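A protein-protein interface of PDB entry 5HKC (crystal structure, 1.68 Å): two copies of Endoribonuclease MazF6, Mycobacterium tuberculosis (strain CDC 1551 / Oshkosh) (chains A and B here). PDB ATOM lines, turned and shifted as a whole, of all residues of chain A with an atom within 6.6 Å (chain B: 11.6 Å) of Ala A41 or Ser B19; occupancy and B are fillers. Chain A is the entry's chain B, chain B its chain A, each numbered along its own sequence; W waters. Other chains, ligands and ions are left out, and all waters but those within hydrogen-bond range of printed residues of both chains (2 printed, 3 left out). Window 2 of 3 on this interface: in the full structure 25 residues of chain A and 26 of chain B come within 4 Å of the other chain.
O of Ala A41 lies within hydrogen-bond range of N of Lys A86 (2.9 Å).
OG1 of Thr B79 lies within hydrogen-bond range of OD1 of Asn B77 (2.6 Å).
The backbone NH (N) of Val B47 is in hydrogen-bond range of the backbone carbonyl oxygen (O) of Ala B80, 2.9 Å away.
Printed residues of chain A that touch a printed residue of chain B: Ala A41, Thr A42, Thr A83 and Asn A85.
Among the printed residues, 11 pairs touch across the chains.
Among the printed residues, no Asp or Glu carboxylate lies within 4 Å of a Lys or Arg side-chain nitrogen of the other chain.
The backbone carbonyl oxygen (O) of Ser B17 sits at hydrogen-bond distance from the side-chain amide nitrogen (ND2) of Asn A85 (2.8 Å).
The backbone NH (N) of Ser B19 lies within hydrogen-bond range of the side-chain amide oxygen (OD1) of Asn A85, 2.8 Å away.
The backbone NH (N) of Gln B20 lies within hydrogen-bond range of the side-chain amide oxygen (OD1) of Asn A85 (3.5 Å).
The side-chain hydroxyl (OG1) of Thr A83 is in hydrogen-bond range of the backbone carbonyl oxygen (O) of Ile B81.
Of the printed residues of chain B, Ala A41 touches Ser B19 (3.3 Å).
Thr A42 touches just one residue of chain B: Ser B19 (3.6 Å).
No residue of chain B comes within 4 Å of Val A43.
Asn A85 touches just these residues of chain B: Ser B17 (2.8 Å), Gly B18 (3.7 Å), Ser B19 (2.8 Å) and Gln B20 (3.5 Å).
No residue of chain B comes within 4 Å of Lys A86.
Printed residues of chain A within 4 Å of Gly B18: Asn A85.
Of chain A, only Ala A41 (3.3 Å), Thr A42 (3.6 Å) and Asn A85 (2.8 Å) come within 4 Å of Ser B19.
Of the printed residues of chain A, Pro B21 touches Thr A83 (3.8 Å).
Val B78 touches none of the printed residues of chain A.
The nearest residue of chain B that does not touch Ala A41 is Gly B18 (6.5 Å).
Ser B19 touches Ala A41 (OG to CB, 3.3 Å).
Thr A42 touches Ser B19.
Gln B20 touches Thr A83.
Thr A83 touches Pro B21 (CB to CD, 3.8 Å).
Thr A83 touches Thr B79 (CG2 to O, 3.6 Å).
Thr A83 touches Ala B80 (OG1 to C, 3.8 Å).
Gly B18 touches Asn A85.
Water W2 bridges the side-chain hydroxyl of Thr A42 (2.6 Å) and the backbone carbonyl oxygen of Thr B79 (2.9 Å).
Water W1 lies within hydrogen-bond range of the side-chain hydroxyl (OG1) of Thr A42 (2.7 Å) and the backbone carbonyl oxygen (O) of Thr B79 (3.2 Å).
No position is printed for both chains.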
ATOM      1  N   SER A  38      22.739  39.720 -20.271  1.00  0.00           N
ATOM      2  CA  SER A  38      22.338  40.287 -21.553  1.00  0.00           C
ATOM      3  C   SER A  38      20.951  39.835 -21.960  1.00  0.00           C
ATOM      4  O   SER A  38      20.320  39.039 -21.267  1.00  0.00           O
ATOM      5  CB  SER A  38      23.340  39.912 -22.640  1.00  0.00           C
ATOM      6  OG  SER A  38      23.083  38.610 -23.139  1.00  0.00           O
ATOM      7  N   ARG A  39      20.493  40.348 -23.097  1.00  0.00           N
ATOM      8  CA  ARG A  39      19.192  40.005 -23.654  1.00  0.00           C
ATOM      9  C   ARG A  39      19.179  38.623 -24.301  1.00  0.00           C
ATOM     10  O   ARG A  39      18.128  38.158 -24.758  1.00  0.00           O
ATOM     11  CB  ARG A  39      18.767  41.060 -24.680  1.00  0.00           C
ATOM     12  CG  ARG A  39      17.615  41.943 -24.229  1.00  0.00           C
ATOM     13  CD  ARG A  39      16.325  41.555 -24.944  1.00  0.00           C
ATOM     14  NE  ARG A  39      16.485  41.577 -26.398  1.00  0.00           N
ATOM     15  CZ  ARG A  39      15.628  41.035 -27.260  1.00  0.00           C
ATOM     16  NH1 ARG A  39      14.539  40.417 -26.821  1.00  0.00           N
ATOM     17  NH2 ARG A  39      15.864  41.107 -28.563  1.00  0.00           N
ATOM     18  N   LEU A  40      20.351  37.988 -24.366  1.00  0.00           N
ATOM     19  CA  LEU A  40      20.460  36.607 -24.833  1.00  0.00           C
ATOM     20  C   LEU A  40      19.392  35.768 -24.146  1.00  0.00           C
ATOM     21  O   LEU A  40      19.257  35.815 -22.934  1.00  0.00           O
ATOM     22  CB  LEU A  40      21.860  36.054 -24.540  1.00  0.00           C
ATOM     23  CG  LEU A  40      22.185  34.627 -24.982  1.00  0.00           C
ATOM     24  CD1 LEU A  40      22.037  34.489 -26.487  1.00  0.00           C
ATOM     25  CD2 LEU A  40      23.591  34.244 -24.518  1.00  0.00           C
ATOM     26  N   ALA A  41      18.614  35.019 -24.918  1.00  0.00           N
ATOM     27  CA  ALA A  41      17.474  34.315 -24.354  1.00  0.00           C
ATOM     28  C   ALA A  41      17.876  33.017 -23.671  1.00  0.00           C
ATOM     29  O   ALA A  41      17.059  32.388 -23.014  1.00  0.00           O
ATOM     30  CB  ALA A  41      16.429  34.037 -25.433  1.00  0.00           C
ATOM     31  N   THR A  42      19.122  32.603 -23.869  1.00  0.00           N
ATOM     32  CA  THR A  42      19.550  31.280 -23.426  1.00  0.00           C
ATOM     33  C   THR A  42      20.679  31.329 -22.400  1.00  0.00           C
ATOM     34  O   THR A  42      21.302  32.365 -22.193  1.00  0.00           O
ATOM     35  CB  THR A  42      20.028  30.429 -24.616  1.00  0.00           C
ATOM     36  OG1 THR A  42      21.039  31.142 -25.325  1.00  0.00           O
ATOM     37  CG2 THR A  42      18.875  30.120 -25.577  1.00  0.00           C
ATOM     38  N   VAL A  43      20.919  30.192 -21.762  1.00  0.00           N
ATOM     39  CA  VAL A  43      22.046  30.023 -20.852  1.00  0.00           C
ATOM     40  C   VAL A  43      22.626  28.632 -21.078  1.00  0.00           C
ATOM     41  O   VAL A  43      21.900  27.680 -21.359  1.00  0.00           O
ATOM     42  CB  VAL A  43      21.648  30.169 -19.369  1.00  0.00           C
ATOM     43  CG1 VAL A  43      21.442  31.623 -19.005  1.00  0.00           C
ATOM     44  CG2 VAL A  43      20.393  29.350 -19.082  1.00  0.00           C
ATOM     45  N   THR A  83      22.219  23.936 -23.768  1.00  0.00           N
ATOM     46  CA  THR A  83      21.858  25.332 -23.905  1.00  0.00           C
ATOM     47  C   THR A  83      20.357  25.410 -23.696  1.00  0.00           C
ATOM     48  O   THR A  83      19.604  24.809 -24.448  1.00  0.00           O
ATOM     49  CB  THR A  83      22.246  25.881 -25.277  1.00  0.00           C
ATOM     50  OG1 THR A  83      23.657  25.726 -25.464  1.00  0.00           O
ATOM     51  CG2 THR A  83      21.858  27.359 -25.410  1.00  0.00           C
ATOM     52  N   LEU A  84      19.940  26.156 -22.676  1.00  0.00           N
ATOM     53  CA  LEU A  84      18.554  26.166 -22.225  1.00  0.00           C
ATOM     54  C   LEU A  84      17.947  27.550 -22.349  1.00  0.00           C
ATOM     55  O   LEU A  84      18.657  28.538 -22.278  1.00  0.00           O
ATOM     56  CB  LEU A  84      18.475  25.722 -20.769  1.00  0.00           C
ATOM     57  CG  LEU A  84      19.030  24.328 -20.483  1.00  0.00           C
ATOM     58  CD1 LEU A  84      19.120  24.100 -18.983  1.00  0.00           C
ATOM     59  CD2 LEU A  84      18.156  23.271 -21.131  1.00  0.00           C
ATOM     60  N   ASN A  85      16.631  27.616 -22.505  1.00  0.00           N
ATOM     61  CA  ASN A  85      15.931  28.887 -22.383  1.00  0.00           C
ATOM     62  C   ASN A  85      16.059  29.361 -20.943  1.00  0.00           C
ATOM     63  O   ASN A  85      15.891  28.569 -20.011  1.00  0.00           O
ATOM     64  CB  ASN A  85      14.465  28.721 -22.754  1.00  0.00           C
ATOM     65  CG  ASN A  85      14.268  28.476 -24.224  1.00  0.00           C
ATOM     66  OD1 ASN A  85      14.801  29.206 -25.063  1.00  0.00           O
ATOM     67  ND2 ASN A  85      13.600  27.375 -24.546  1.00  0.00           N
ATOM     68  N   LYS A  86      16.368  30.635 -20.756  1.00  0.00           N
ATOM     69  CA  LYS A  86      16.462  31.180 -19.406  1.00  0.00           C
ATOM     70  C   LYS A  86      15.186  30.886 -18.616  1.00  0.00           C
ATOM     71  O   LYS A  86      15.233  30.653 -17.403  1.00  0.00           O
ATOM     72  CB  LYS A  86      16.741  32.679 -19.450  1.00  0.00           C
ATOM     73  CG  LYS A  86      18.165  33.033 -19.819  1.00  0.00           C
ATOM     74  CD  LYS A  86      18.363  34.538 -19.843  1.00  0.00           C
ATOM     75  CE  LYS A  86      19.817  34.900 -20.039  1.00  0.00           C
ATOM     76  NZ  LYS A  86      19.982  36.368 -20.375  1.00  0.00           N
ATOM     77  N   THR A  87      14.056  30.871 -19.325  1.00  0.00           N
ATOM     78  CA  THR A  87      12.758  30.598 -18.714  1.00  0.00           C
ATOM     79  C   THR A  87      12.573  29.137 -18.302  1.00  0.00           C
ATOM     80  O   THR A  87      11.640  28.813 -17.568  1.00  0.00           O
ATOM     81  CB  THR A  87      11.603  31.002 -19.664  1.00  0.00           C
ATOM     82  OG1 THR A  87      11.707  30.278 -20.898  1.00  0.00           O
ATOM     83  CG2 THR A  87      11.648  32.496 -19.954  1.00  0.00           C
ATOM     84  N   LEU B  13      18.878  18.706 -34.715  1.00  0.00           N
ATOM     85  CA  LEU B  13      18.860  19.171 -33.336  1.00  0.00           C
ATOM     86  C   LEU B  13      17.455  19.154 -32.761  1.00  0.00           C
ATOM     87  O   LEU B  13      17.248  19.516 -31.602  1.00  0.00           O
ATOM     88  CB  LEU B  13      19.458  20.577 -33.237  1.00  0.00           C
ATOM     89  CG  LEU B  13      20.899  20.720 -33.738  1.00  0.00           C
ATOM     90  CD1 LEU B  13      21.423  22.104 -33.386  1.00  0.00           C
ATOM     91  CD2 LEU B  13      21.801  19.655 -33.150  1.00  0.00           C
ATOM     92  N   GLY B  14      16.491  18.743 -33.581  1.00  0.00           N
ATOM     93  CA  GLY B  14      15.137  18.532 -33.099  1.00  0.00           C
ATOM     94  C   GLY B  14      14.234  19.744 -33.166  1.00  0.00           C
ATOM     95  O   GLY B  14      14.580  20.764 -33.762  1.00  0.00           O
ATOM     96  N   PRO B  15      13.064  19.645 -32.520  1.00  0.00           N
ATOM     97  CA  PRO B  15      12.008  20.649 -32.625  1.00  0.00           C
ATOM     98  C   PRO B  15      12.386  21.954 -31.961  1.00  0.00           C
ATOM     99  O   PRO B  15      13.072  21.936 -30.941  1.00  0.00           O
ATOM    100  CB  PRO B  15      10.822  20.008 -31.884  1.00  0.00           C
ATOM    101  CG  PRO B  15      11.225  18.618 -31.577  1.00  0.00           C
ATOM    102  CD  PRO B  15      12.714  18.581 -31.573  1.00  0.00           C
ATOM    103  N   PRO B  16      11.930  23.077 -32.517  1.00  0.00           N
ATOM    104  CA  PRO B  16      12.238  24.313 -31.798  1.00  0.00           C
ATOM    105  C   PRO B  16      11.553  24.359 -30.434  1.00  0.00           C
ATOM    106  O   PRO B  16      10.549  23.682 -30.184  1.00  0.00           O
ATOM    107  CB  PRO B  16      11.687  25.407 -32.721  1.00  0.00           C
ATOM    108  CG  PRO B  16      11.636  24.769 -34.090  1.00  0.00           C
ATOM    109  CD  PRO B  16      11.320  23.322 -33.835  1.00  0.00           C
ATOM    110  N   SER B  17      12.158  25.107 -29.526  1.00  0.00           N
ATOM    111  CA  SER B  17      11.584  25.320 -28.212  1.00  0.00           C
ATOM    112  C   SER B  17      12.157  26.634 -27.722  1.00  0.00           C
ATOM    113  O   SER B  17      13.267  26.664 -27.209  1.00  0.00           O
ATOM    114  CB  SER B  17      11.882  24.164 -27.265  1.00  0.00           C
ATOM    115  OG  SER B  17      11.208  24.338 -26.032  1.00  0.00           O
ATOM    116  N   GLY B  18      11.440  27.726 -27.953  1.00  0.00           N
ATOM    117  CA  GLY B  18      11.945  29.046 -27.634  1.00  0.00           C
ATOM    118  C   GLY B  18      13.199  29.320 -28.441  1.00  0.00           C
ATOM    119  O   GLY B  18      13.192  29.196 -29.676  1.00  0.00           O
ATOM    120  N   SER B  19      14.276  29.681 -27.747  1.00  0.00           N
ATOM    121  CA  SER B  19      15.534  30.053 -28.393  1.00  0.00           C
ATOM    122  C   SER B  19      16.597  28.949 -28.375  1.00  0.00           C
ATOM    123  O   SER B  19      17.721  29.177 -28.802  1.00  0.00           O
ATOM    124  CB  SER B  19      16.110  31.318 -27.754  1.00  0.00           C
ATOM    125  OG  SER B  19      15.367  32.465 -28.139  1.00  0.00           O
ATOM    126  N   GLN B  20      16.270  27.780 -27.841  1.00  0.00           N
ATOM    127  CA  GLN B  20      17.293  26.736 -27.737  1.00  0.00           C
ATOM    128  C   GLN B  20      17.649  26.178 -29.114  1.00  0.00           C
ATOM    129  O   GLN B  20      16.877  26.348 -30.085  1.00  0.00           O
ATOM    130  CB  GLN B  20      16.852  25.606 -26.798  1.00  0.00           C
ATOM    131  CG  GLN B  20      15.738  24.749 -27.254  1.00  0.00           C
ATOM    132  CD  GLN B  20      15.234  23.882 -26.109  1.00  0.00           C
ATOM    133  OE1 GLN B  20      15.538  24.146 -24.947  1.00  0.00           O
ATOM    134  NE2 GLN B  20      14.549  22.800 -26.438  1.00  0.00           N
ATOM    135  N   PRO B  21      18.843  25.576 -29.233  1.00  0.00           N
ATOM    136  CA  PRO B  21      19.273  25.074 -30.536  1.00  0.00           C
ATOM    137  C   PRO B  21      18.237  24.093 -31.089  1.00  0.00           C
ATOM    138  O   PRO B  21      17.663  23.287 -30.349  1.00  0.00           O
ATOM    139  CB  PRO B  21      20.588  24.359 -30.210  1.00  0.00           C
ATOM    140  CG  PRO B  21      21.116  25.082 -29.001  1.00  0.00           C
ATOM    141  CD  PRO B  21      19.875  25.371 -28.194  1.00  0.00           C
ATOM    142  N   ALA B  22      18.031  24.139 -32.397  1.00  0.00           N
ATOM    143  CA  ALA B  22      17.019  23.291 -33.013  1.00  0.00           C
ATOM    144  C   ALA B  22      17.235  23.169 -34.504  1.00  0.00           C
ATOM    145  O   ALA B  22      18.071  23.882 -35.079  1.00  0.00           O
ATOM    146  CB  ALA B  22      15.623  23.838 -32.722  1.00  0.00           C
ATOM    147  N   LYS B  23      16.510  22.211 -35.089  1.00  0.00           N
ATOM    148  CA  LYS B  23      16.461  21.990 -36.534  1.00  0.00           C
ATOM    149  C   LYS B  23      17.732  21.330 -37.064  1.00  0.00           C
ATOM    150  O   LYS B  23      18.703  21.167 -36.339  1.00  0.00           O
ATOM    151  CB  LYS B  23      16.170  23.314 -37.254  1.00  0.00           C
ATOM    152  CG  LYS B  23      14.782  23.844 -36.949  1.00  0.00           C
ATOM    153  CD  LYS B  23      14.652  25.317 -37.302  1.00  0.00           C
ATOM    154  CE  LYS B  23      15.173  25.611 -38.689  1.00  0.00           C
ATOM    155  NZ  LYS B  23      14.817  26.998 -39.125  1.00  0.00           N
ATOM    156  N   ARG B  25      21.080  21.272 -38.911  1.00  0.00           N
ATOM    157  CA  ARG B  25      22.068  22.308 -39.188  1.00  0.00           C
ATOM    158  C   ARG B  25      23.476  21.756 -39.126  1.00  0.00           C
ATOM    159  O   ARG B  25      23.670  20.652 -38.629  1.00  0.00           O
ATOM    160  CB  ARG B  25      21.921  23.451 -38.205  1.00  0.00           C
ATOM    161  CG  ARG B  25      22.142  23.067 -36.790  1.00  0.00           C
ATOM    162  CD  ARG B  25      21.890  24.283 -35.939  1.00  0.00           C
ATOM    163  NE  ARG B  25      20.536  24.800 -36.081  1.00  0.00           N
ATOM    164  CZ  ARG B  25      20.199  25.860 -36.815  1.00  0.00           C
ATOM    165  NH1 ARG B  25      21.126  26.533 -37.492  1.00  0.00           N
ATOM    166  NH2 ARG B  25      18.931  26.235 -36.884  1.00  0.00           N
ATOM    167  N   VAL B  47      26.790  25.208 -32.468  1.00  0.00           N
ATOM    168  CA  VAL B  47      25.864  25.381 -33.589  1.00  0.00           C
ATOM    169  C   VAL B  47      26.408  26.356 -34.620  1.00  0.00           C
ATOM    170  O   VAL B  47      26.989  27.380 -34.273  1.00  0.00           O
ATOM    171  CB  VAL B  47      24.517  25.893 -33.076  1.00  0.00           C
ATOM    172  CG1 VAL B  47      23.651  26.435 -34.206  1.00  0.00           C
ATOM    173  CG2 VAL B  47      23.823  24.831 -32.228  1.00  0.00           C
ATOM    174  N   ILE B  48      26.249  25.997 -35.888  1.00  0.00           N
ATOM    175  CA  ILE B  48      26.595  26.868 -37.003  1.00  0.00           C
ATOM    176  C   ILE B  48      25.318  27.382 -37.664  1.00  0.00           C
ATOM    177  O   ILE B  48      24.338  26.642 -37.803  1.00  0.00           O
ATOM    178  CB  ILE B  48      27.481  26.133 -38.037  1.00  0.00           C
ATOM    179  CG1 ILE B  48      28.872  25.881 -37.459  1.00  0.00           C
ATOM    180  CG2 ILE B  48      27.615  26.945 -39.317  1.00  0.00           C
ATOM    181  CD1 ILE B  48      29.704  24.913 -38.279  1.00  0.00           C
ATOM    182  N   THR B  49      25.294  28.662 -38.003  1.00  0.00           N
ATOM    183  CA  THR B  49      24.127  29.215 -38.678  1.00  0.00           C
ATOM    184  C   THR B  49      24.555  30.071 -39.876  1.00  0.00           C
ATOM    185  O   THR B  49      25.676  30.576 -39.915  1.00  0.00           O
ATOM    186  CB  THR B  49      23.296  30.058 -37.702  1.00  0.00           C
ATOM    187  OG1 THR B  49      22.188  30.647 -38.387  1.00  0.00           O
ATOM    188  CG2 THR B  49      24.154  31.156 -37.106  1.00  0.00           C
ATOM    189  N   ASN B  51      22.949  32.744 -40.541  1.00  0.00           N
ATOM    190  CA  ASN B  51      22.430  34.054 -40.173  1.00  0.00           C
ATOM    191  C   ASN B  51      23.561  35.039 -39.900  1.00  0.00           C
ATOM    192  O   ASN B  51      24.180  35.008 -38.834  1.00  0.00           O
ATOM    193  CB  ASN B  51      21.516  33.956 -38.953  1.00  0.00           C
ATOM    194  CG  ASN B  51      20.767  35.249 -38.677  1.00  0.00           C
ATOM    195  OD1 ASN B  51      21.054  36.291 -39.274  1.00  0.00           O
ATOM    196  ND2 ASN B  51      19.805  35.189 -37.769  1.00  0.00           N
ATOM    197  N   LEU B  54      24.423  37.090 -36.509  1.00  0.00           N
ATOM    198  CA  LEU B  54      25.111  36.525 -35.353  1.00  0.00           C
ATOM    199  C   LEU B  54      26.624  36.638 -35.433  1.00  0.00           C
ATOM    200  O   LEU B  54      27.317  36.376 -34.455  1.00  0.00           O
ATOM    201  CB  LEU B  54      24.704  35.065 -35.153  1.00  0.00           C
ATOM    202  CG  LEU B  54      23.219  34.933 -34.823  1.00  0.00           C
ATOM    203  CD1 LEU B  54      22.754  33.507 -34.965  1.00  0.00           C
ATOM    204  CD2 LEU B  54      22.959  35.435 -33.410  1.00  0.00           C
ATOM    205  N   MET B  57      27.985  39.087 -32.855  1.00  0.00           N
ATOM    206  CA  MET B  57      27.977  38.787 -31.428  1.00  0.00           C
ATOM    207  C   MET B  57      29.398  38.473 -30.970  1.00  0.00           C
ATOM    208  O   MET B  57      30.087  37.692 -31.612  1.00  0.00           O
ATOM    209  CB  MET B  57      27.034  37.625 -31.116  1.00  0.00           C
ATOM    210  CG  MET B  57      27.005  37.240 -29.641  1.00  0.00           C
ATOM    211  SD  MET B  57      25.751  35.999 -29.290  1.00  0.00           S
ATOM    212  CE  MET B  57      24.249  36.908 -29.628  1.00  0.00           C
ATOM    213  N   ASN B  77      28.171  29.896 -33.645  1.00  0.00           N
ATOM    214  CA  ASN B  77      27.518  30.545 -32.515  1.00  0.00           C
ATOM    215  C   ASN B  77      27.954  29.891 -31.214  1.00  0.00           C
ATOM    216  O   ASN B  77      27.440  28.836 -30.844  1.00  0.00           O
ATOM    217  CB  ASN B  77      25.999  30.477 -32.654  1.00  0.00           C
ATOM    218  CG  ASN B  77      25.279  31.285 -31.600  1.00  0.00           C
ATOM    219  OD1 ASN B  77      25.900  31.908 -30.726  1.00  0.00           O
ATOM    220  ND2 ASN B  77      23.950  31.282 -31.670  1.00  0.00           N
ATOM    221  N   VAL B  78      28.919  30.510 -30.538  1.00  0.00           N
ATOM    222  CA  VAL B  78      29.511  29.911 -29.340  1.00  0.00           C
ATOM    223  C   VAL B  78      28.591  30.028 -28.133  1.00  0.00           C
ATOM    224  O   VAL B  78      28.874  29.456 -27.085  1.00  0.00           O
ATOM    225  CB  VAL B  78      30.884  30.540 -28.999  1.00  0.00           C
ATOM    226  CG1 VAL B  78      31.904  30.172 -30.071  1.00  0.00           C
ATOM    227  CG2 VAL B  78      30.768  32.039 -28.871  1.00  0.00           C
ATOM    228  N   THR B  79      27.476  30.744 -28.279  1.00  0.00           N
ATOM    229  CA  THR B  79      26.485  30.776 -27.215  1.00  0.00           C
ATOM    230  C   THR B  79      25.475  29.638 -27.381  1.00  0.00           C
ATOM    231  O   THR B  79      24.560  29.491 -26.567  1.00  0.00           O
ATOM    232  CB  THR B  79      25.706  32.114 -27.172  1.00  0.00           C
ATOM    233  OG1 THR B  79      24.913  32.238 -28.362  1.00  0.00           O
ATOM    234  CG2 THR B  79      26.654  33.298 -27.050  1.00  0.00           C
ATOM    235  N   ALA B  80      25.650  28.837 -28.430  1.00  0.00           N
ATOM    236  CA  ALA B  80      24.730  27.739 -28.734  1.00  0.00           C
ATOM    237  C   ALA B  80      25.463  26.399 -28.785  1.00  0.00           C
ATOM    238  O   ALA B  80      25.969  25.990 -29.829  1.00  0.00           O
ATOM    239  CB  ALA B  80      24.002  28.001 -30.048  1.00  0.00           C
ATOM    240  N   ILE B  81      25.529  25.735 -27.639  1.00  0.00           N
ATOM    241  CA  ILE B  81      26.301  24.498 -27.490  1.00  0.00           C
ATOM    242  C   ILE B  81      25.361  23.317 -27.258  1.00  0.00           C
ATOM    243  O   ILE B  81      24.419  23.426 -26.476  1.00  0.00           O
ATOM    244  CB  ILE B  81      27.313  24.644 -26.328  1.00  0.00           C
ATOM    245  CG1 ILE B  81      28.252  25.831 -26.601  1.00  0.00           C
ATOM    246  CG2 ILE B  81      28.080  23.357 -26.116  1.00  0.00           C
ATOM    247  CD1 ILE B  81      29.373  25.997 -25.554  1.00  0.00           C
ATOM    248  N   VAL B  82      25.592  22.215 -27.969  1.00  0.00           N
ATOM    249  CA  VAL B  82      24.740  21.042 -27.834  1.00  0.00           C
ATOM    250  C   VAL B  82      25.578  19.820 -27.532  1.00  0.00           C
ATOM    251  O   VAL B  82      26.757  19.757 -27.890  1.00  0.00           O
ATOM    252  CB  VAL B  82      23.916  20.776 -29.103  1.00  0.00           C
ATOM    253  CG1 VAL B  82      22.916  21.887 -29.333  1.00  0.00           C
ATOM    254  CG2 VAL B  82      24.838  20.582 -30.310  1.00  0.00           C
HETATM  255  O   HOH W   1      21.791  30.575 -27.827  1.00  0.00           O
HETATM  256  O   HOH W   2      23.406  30.684 -24.232  1.00  0.00           O
